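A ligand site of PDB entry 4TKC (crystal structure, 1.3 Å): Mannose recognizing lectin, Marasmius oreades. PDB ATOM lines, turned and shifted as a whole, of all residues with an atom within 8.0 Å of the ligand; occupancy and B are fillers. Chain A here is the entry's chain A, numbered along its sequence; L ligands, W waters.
OH of Tyr 104 is in hydrogen-bond range of O4 of the ligand (2.7 Å).
An oxygen (O2) of the ligand is in hydrogen-bond range of the side-chain carboxylate (OD2) of Asp 98, at 2.7 Å.
An oxygen (O3) of the ligand is in hydrogen-bond range of the side-chain amide oxygen of Gln 96.
The side-chain amide nitrogen (ND2) of Asn 100 lies within hydrogen-bond range of an oxygen (O2) of the ligand.
The side-chain hydroxyl of Thr 114 sits at hydrogen-bond distance from the side-chain amide oxygen of Asn 100 (3.2 Å).
The side-chain amide oxygen (OE1) of Gln 96 lies close to the side-chain carboxylate (OD1) of Asp 98, 3.2 Å away.
The side-chain hydroxyl (OH) of Tyr 104 is in hydrogen-bond range of the side-chain amide nitrogen (NE2) of Gln 96, at 2.6 Å.
OD1 of Asn 100 lies within hydrogen-bond range of N of Thr 116, 3.1 Å away.
The side-chain carboxylate (OD1) of Asp 98 sits at hydrogen-bond distance from the backbone NH (N) of Asn 100, at 3.0 Å.
N of Val 118 sits at hydrogen-bond distance from O of Asp 98 (2.8 Å).
The backbone NH (N) of Asn 115 sits at hydrogen-bond distance from the side-chain amide oxygen (OD1) of Asn 100 (3.0 Å).
Ala 110 touches the ligand (CB to C6, 3.7 Å).
His 113 touches the ligand.
Ala 117 touches the ligand.
Hydrophobic or aromatic side chains within 4 Å of the ligand: Tyr 104, Ala 110, His 113 and Ala 117.
Water W1 lies within hydrogen-bond range of OD2 of Asp 98 (2.8 Å) and O3 of the ligand (3.5 Å).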
ATOM      1  N   VAL A  94      10.828  32.914  26.563  1.00  0.00           N
ATOM      2  CA  VAL A  94       9.562  32.723  25.908  1.00  0.00           C
ATOM      3  C   VAL A  94       9.217  31.230  25.783  1.00  0.00           C
ATOM      4  O   VAL A  94      10.013  30.404  25.268  1.00  0.00           O
ATOM      5  CB  VAL A  94       9.530  33.345  24.484  1.00  0.00           C
ATOM      6  CG1 VAL A  94       8.157  33.208  23.863  1.00  0.00           C
ATOM      7  CG2 VAL A  94       9.895  34.816  24.538  1.00  0.00           C
ATOM      8  N   GLN A  96       7.126  28.848  23.792  1.00  0.00           N
ATOM      9  CA  GLN A  96       6.536  28.973  22.446  1.00  0.00           C
ATOM     10  C   GLN A  96       5.566  27.829  22.105  1.00  0.00           C
ATOM     11  O   GLN A  96       5.679  26.714  22.678  1.00  0.00           O
ATOM     12  CB  GLN A  96       7.642  29.026  21.393  1.00  0.00           C
ATOM     13  CG  GLN A  96       8.546  30.243  21.515  1.00  0.00           C
ATOM     14  CD  GLN A  96       9.656  30.360  20.501  1.00  0.00           C
ATOM     15  OE1 GLN A  96       9.978  29.375  19.758  1.00  0.00           O
ATOM     16  NE2 GLN A  96      10.103  31.550  20.254  1.00  0.00           N
ATOM     17  N   ASN A  97       4.658  28.118  21.171  1.00  0.00           N
ATOM     18  CA  ASN A  97       3.735  27.122  20.669  1.00  0.00           C
ATOM     19  C   ASN A  97       4.453  25.913  20.025  1.00  0.00           C
ATOM     20  O   ASN A  97       3.944  24.801  20.131  1.00  0.00           O
ATOM     21  CB  ASN A  97       2.799  27.693  19.613  1.00  0.00           C
ATOM     22  CG  ASN A  97       1.826  28.702  20.136  1.00  0.00           C
ATOM     23  OD1 ASN A  97       1.527  28.767  21.338  1.00  0.00           O
ATOM     24  ND2 ASN A  97       1.272  29.494  19.229  1.00  0.00           N
ATOM     25  N   ASP A  98       5.677  26.116  19.552  1.00  0.00           N
ATOM     26  CA  ASP A  98       6.386  24.992  18.898  1.00  0.00           C
ATOM     27  C   ASP A  98       7.014  24.031  19.906  1.00  0.00           C
ATOM     28  O   ASP A  98       7.526  22.947  19.479  1.00  0.00           O
ATOM     29  CB  ASP A  98       7.375  25.461  17.839  1.00  0.00           C
ATOM     30  CG  ASP A  98       8.570  26.206  18.376  1.00  0.00           C
ATOM     31  OD1 ASP A  98       8.691  26.448  19.612  1.00  0.00           O
ATOM     32  OD2 ASP A  98       9.354  26.679  17.492  1.00  0.00           O
ATOM     33  N   GLY A  99       6.958  24.440  21.206  1.00  0.00           N
ATOM     34  CA  GLY A  99       7.449  23.577  22.256  1.00  0.00           C
ATOM     35  C   GLY A  99       8.785  24.020  22.813  1.00  0.00           C
ATOM     36  O   GLY A  99       9.283  23.488  23.816  1.00  0.00           O
ATOM     37  N   ASN A 100       9.420  24.917  22.071  1.00  0.00           N
ATOM     38  CA  ASN A 100      10.729  25.391  22.444  1.00  0.00           C
ATOM     39  C   ASN A 100      10.593  26.465  23.540  1.00  0.00           C
ATOM     40  O   ASN A 100       9.675  27.292  23.462  1.00  0.00           O
ATOM     41  CB  ASN A 100      11.459  25.993  21.253  1.00  0.00           C
ATOM     42  CG  ASN A 100      12.933  25.636  21.195  1.00  0.00           C
ATOM     43  OD1 ASN A 100      13.456  24.974  22.100  1.00  0.00           O
ATOM     44  ND2 ASN A 100      13.601  26.073  20.134  1.00  0.00           N
ATOM     45  N   LEU A 101      11.534  26.431  24.474  1.00  0.00           N
ATOM     46  CA  LEU A 101      11.600  27.480  25.549  1.00  0.00           C
ATOM     47  C   LEU A 101      12.927  28.181  25.219  1.00  0.00           C
ATOM     48  O   LEU A 101      13.999  27.554  25.186  1.00  0.00           O
ATOM     49  CB  LEU A 101      11.628  26.809  26.892  1.00  0.00           C
ATOM     50  CG  LEU A 101      11.711  27.807  28.072  1.00  0.00           C
ATOM     51  CD1 LEU A 101      10.381  28.519  28.302  1.00  0.00           C
ATOM     52  CD2 LEU A 101      12.152  27.063  29.317  1.00  0.00           C
ATOM     53  N   VAL A 102      12.848  29.501  25.018  1.00  0.00           N
ATOM     54  CA  VAL A 102      13.918  30.260  24.445  1.00  0.00           C
ATOM     55  C   VAL A 102      14.225  31.528  25.265  1.00  0.00           C
ATOM     56  O   VAL A 102      13.308  32.297  25.595  1.00  0.00           O
ATOM     57  CB  VAL A 102      13.586  30.676  22.976  1.00  0.00           C
ATOM     58  CG1 VAL A 102      14.799  31.284  22.303  1.00  0.00           C
ATOM     59  CG2 VAL A 102      13.072  29.505  22.137  1.00  0.00           C
ATOM     60  N   VAL A 103      15.523  31.764  25.520  1.00  0.00           N
ATOM     61  CA  VAL A 103      16.001  33.085  26.011  1.00  0.00           C
ATOM     62  C   VAL A 103      16.397  33.894  24.793  1.00  0.00           C
ATOM     63  O   VAL A 103      17.313  33.498  24.035  1.00  0.00           O
ATOM     64  CB  VAL A 103      17.198  33.008  26.968  1.00  0.00           C
ATOM     65  CG1 VAL A 103      17.630  34.425  27.348  1.00  0.00           C
ATOM     66  CG2 VAL A 103      16.863  32.198  28.217  1.00  0.00           C
ATOM     67  N   TYR A 104      15.637  34.933  24.512  1.00  0.00           N
ATOM     68  CA  TYR A 104      15.897  35.885  23.473  1.00  0.00           C
ATOM     69  C   TYR A 104      16.593  37.139  24.013  1.00  0.00           C
ATOM     70  O   TYR A 104      16.155  37.716  25.035  1.00  0.00           O
ATOM     71  CB  TYR A 104      14.590  36.317  22.797  1.00  0.00           C
ATOM     72  CG  TYR A 104      13.989  35.283  21.854  1.00  0.00           C
ATOM     73  CD1 TYR A 104      14.556  35.007  20.598  1.00  0.00           C
ATOM     74  CD2 TYR A 104      12.892  34.553  22.244  1.00  0.00           C
ATOM     75  CE1 TYR A 104      13.999  34.065  19.775  1.00  0.00           C
ATOM     76  CE2 TYR A 104      12.310  33.636  21.393  1.00  0.00           C
ATOM     77  CZ  TYR A 104      12.894  33.370  20.173  1.00  0.00           C
ATOM     78  OH  TYR A 104      12.362  32.414  19.315  1.00  0.00           O
ATOM     79  N   GLY A 108      15.157  39.705  18.901  1.00  0.00           N
ATOM     80  CA  GLY A 108      14.761  38.312  18.701  1.00  0.00           C
ATOM     81  C   GLY A 108      15.903  37.354  18.436  1.00  0.00           C
ATOM     82  O   GLY A 108      15.686  36.300  17.871  1.00  0.00           O
ATOM     83  N   LYS A 109      17.070  37.634  19.013  1.00  0.00           N
ATOM     84  CA  LYS A 109      18.253  36.766  18.924  1.00  0.00           C
ATOM     85  C   LYS A 109      18.201  35.666  19.987  1.00  0.00           C
ATOM     86  O   LYS A 109      18.264  35.990  21.175  1.00  0.00           O
ATOM     87  CB  LYS A 109      19.537  37.577  19.058  1.00  0.00           C
ATOM     88  CG  LYS A 109      20.850  36.794  19.064  1.00  0.00           C
ATOM     89  CD  LYS A 109      21.025  35.886  17.872  1.00  0.00           C
ATOM     90  CE  LYS A 109      22.231  34.974  18.101  1.00  0.00           C
ATOM     91  NZ  LYS A 109      22.431  34.025  16.993  1.00  0.00           N
ATOM     92  N   ALA A 110      18.014  34.403  19.562  1.00  0.00           N
ATOM     93  CA  ALA A 110      17.960  33.300  20.490  1.00  0.00           C
ATOM     94  C   ALA A 110      19.380  33.083  20.990  1.00  0.00           C
ATOM     95  O   ALA A 110      20.290  32.863  20.170  1.00  0.00           O
ATOM     96  CB  ALA A 110      17.399  32.025  19.828  1.00  0.00           C
ATOM     97  N   VAL A 111      19.573  33.171  22.314  1.00  0.00           N
ATOM     98  CA  VAL A 111      20.886  32.903  22.913  1.00  0.00           C
ATOM     99  C   VAL A 111      20.932  31.643  23.816  1.00  0.00           C
ATOM    100  O   VAL A 111      21.984  31.246  24.298  1.00  0.00           O
ATOM    101  CB  VAL A 111      21.400  34.126  23.719  1.00  0.00           C
ATOM    102  CG1 VAL A 111      21.669  35.279  22.775  1.00  0.00           C
ATOM    103  CG2 VAL A 111      20.432  34.620  24.813  1.00  0.00           C
ATOM    104  N   TRP A 112      19.778  31.031  24.003  1.00  0.00           N
ATOM    105  CA  TRP A 112      19.659  29.777  24.709  1.00  0.00           C
ATOM    106  C   TRP A 112      18.273  29.181  24.397  1.00  0.00           C
ATOM    107  O   TRP A 112      17.287  29.897  24.168  1.00  0.00           O
ATOM    108  CB  TRP A 112      19.819  29.959  26.227  1.00  0.00           C
ATOM    109  CG  TRP A 112      19.737  28.695  27.033  1.00  0.00           C
ATOM    110  CD1 TRP A 112      20.778  27.955  27.475  1.00  0.00           C
ATOM    111  CD2 TRP A 112      18.541  28.054  27.535  1.00  0.00           C
ATOM    112  NE1 TRP A 112      20.322  26.869  28.174  1.00  0.00           N
ATOM    113  CE2 TRP A 112      18.960  26.918  28.249  1.00  0.00           C
ATOM    114  CE3 TRP A 112      17.174  28.306  27.401  1.00  0.00           C
ATOM    115  CZ2 TRP A 112      18.046  26.055  28.860  1.00  0.00           C
ATOM    116  CZ3 TRP A 112      16.292  27.444  27.992  1.00  0.00           C
ATOM    117  CH2 TRP A 112      16.730  26.347  28.744  1.00  0.00           C
ATOM    118  N   HIS A 113      18.235  27.861  24.294  1.00  0.00           N
ATOM    119  CA  HIS A 113      16.959  27.199  24.112  1.00  0.00           C
ATOM    120  C   HIS A 113      16.999  25.784  24.660  1.00  0.00           C
ATOM    121  O   HIS A 113      18.084  25.153  24.799  1.00  0.00           O
ATOM    122  CB  HIS A 113      16.506  27.295  22.650  1.00  0.00           C
ATOM    123  CG  HIS A 113      17.214  26.378  21.702  1.00  0.00           C
ATOM    124  ND1 HIS A 113      18.591  26.372  21.565  1.00  0.00           N
ATOM    125  CD2 HIS A 113      16.743  25.481  20.807  1.00  0.00           C
ATOM    126  CE1 HIS A 113      18.923  25.475  20.636  1.00  0.00           C
ATOM    127  NE2 HIS A 113      17.817  24.899  20.203  1.00  0.00           N
ATOM    128  N   THR A 114      15.811  25.265  24.893  1.00  0.00           N
ATOM    129  CA  THR A 114      15.684  23.888  25.336  1.00  0.00           C
ATOM    130  C   THR A 114      15.931  22.878  24.199  1.00  0.00           C
ATOM    131  O   THR A 114      16.079  21.688  24.466  1.00  0.00           O
ATOM    132  CB  THR A 114      14.302  23.610  26.011  1.00  0.00           C
ATOM    133  OG1 THR A 114      13.240  24.084  25.200  1.00  0.00           O
ATOM    134  CG2 THR A 114      14.238  24.253  27.415  1.00  0.00           C
ATOM    135  N   ASN A 115      15.784  23.328  22.953  1.00  0.00           N
ATOM    136  CA  ASN A 115      15.850  22.444  21.779  1.00  0.00           C
ATOM    137  C   ASN A 115      14.733  21.422  21.904  1.00  0.00           C
ATOM    138  O   ASN A 115      14.973  20.240  21.602  1.00  0.00           O
ATOM    139  CB  ASN A 115      17.226  21.741  21.608  1.00  0.00           C
ATOM    140  CG  ASN A 115      17.299  20.944  20.303  1.00  0.00           C
ATOM    141  OD1 ASN A 115      16.786  21.408  19.289  1.00  0.00           O
ATOM    142  ND2 ASN A 115      17.887  19.693  20.317  1.00  0.00           N
ATOM    143  N   THR A 116      13.505  21.909  21.993  1.00  0.00           N
ATOM    144  CA  THR A 116      12.333  21.068  22.161  1.00  0.00           C
ATOM    145  C   THR A 116      11.185  21.618  21.300  1.00  0.00           C
ATOM    146  O   THR A 116       9.988  21.505  21.673  1.00  0.00           O
ATOM    147  CB  THR A 116      11.896  20.952  23.638  1.00  0.00           C
ATOM    148  OG1 THR A 116      11.594  22.264  24.150  1.00  0.00           O
ATOM    149  CG2 THR A 116      12.975  20.342  24.521  1.00  0.00           C
ATOM    150  N   ALA A 117      11.555  22.093  20.086  1.00  0.00           N
ATOM    151  CA  ALA A 117      10.579  22.558  19.073  1.00  0.00           C
ATOM    152  C   ALA A 117       9.965  21.353  18.334  1.00  0.00           C
ATOM    153  O   ALA A 117      10.253  21.067  17.149  1.00  0.00           O
ATOM    154  CB  ALA A 117      11.227  23.547  18.102  1.00  0.00           C
ATOM    155  N   VAL A 118       9.102  20.643  19.053  1.00  0.00           N
ATOM    156  CA  VAL A 118       8.547  19.375  18.618  1.00  0.00           C
ATOM    157  C   VAL A 118       7.221  19.498  17.927  1.00  0.00           C
ATOM    158  O   VAL A 118       6.855  18.582  17.241  1.00  0.00           O
ATOM    159  CB  VAL A 118       8.350  18.381  19.807  1.00  0.00           C
ATOM    160  CG1 VAL A 118       9.698  18.005  20.417  1.00  0.00           C
ATOM    161  CG2 VAL A 118       7.401  18.932  20.869  1.00  0.00           C
HETATM  162  C1  LIG L   1      13.587  27.104  16.521  1.00  0.00           C
HETATM  163  C2  LIG L   1      12.327  27.877  16.906  1.00  0.00           C
HETATM  164  C3  LIG L   1      12.686  29.359  17.017  1.00  0.00           C
HETATM  165  C4  LIG L   1      13.829  29.552  18.020  1.00  0.00           C
HETATM  166  C5  LIG L   1      15.037  28.703  17.594  1.00  0.00           C
HETATM  167  C6  LIG L   1      16.130  28.744  18.637  1.00  0.00           C
HETATM  168  O1  LIG L   1      13.991  27.453  15.210  1.00  0.00           O
HETATM  169  O2  LIG L   1      11.849  27.341  18.105  1.00  0.00           O
HETATM  170  O3  LIG L   1      11.535  30.046  17.466  1.00  0.00           O
HETATM  171  O4  LIG L   1      14.176  30.924  18.076  1.00  0.00           O
HETATM  172  O5  LIG L   1      14.654  27.342  17.396  1.00  0.00           O
HETATM  173  O6  LIG L   1      17.291  28.112  18.141  1.00  0.00           O
HETATM  174  O   HOH W   1       8.357  29.067  16.424  1.00  0.00           O
HETATM  175  O   HOH W   2      15.455  32.248  16.207  1.00  0.00           O
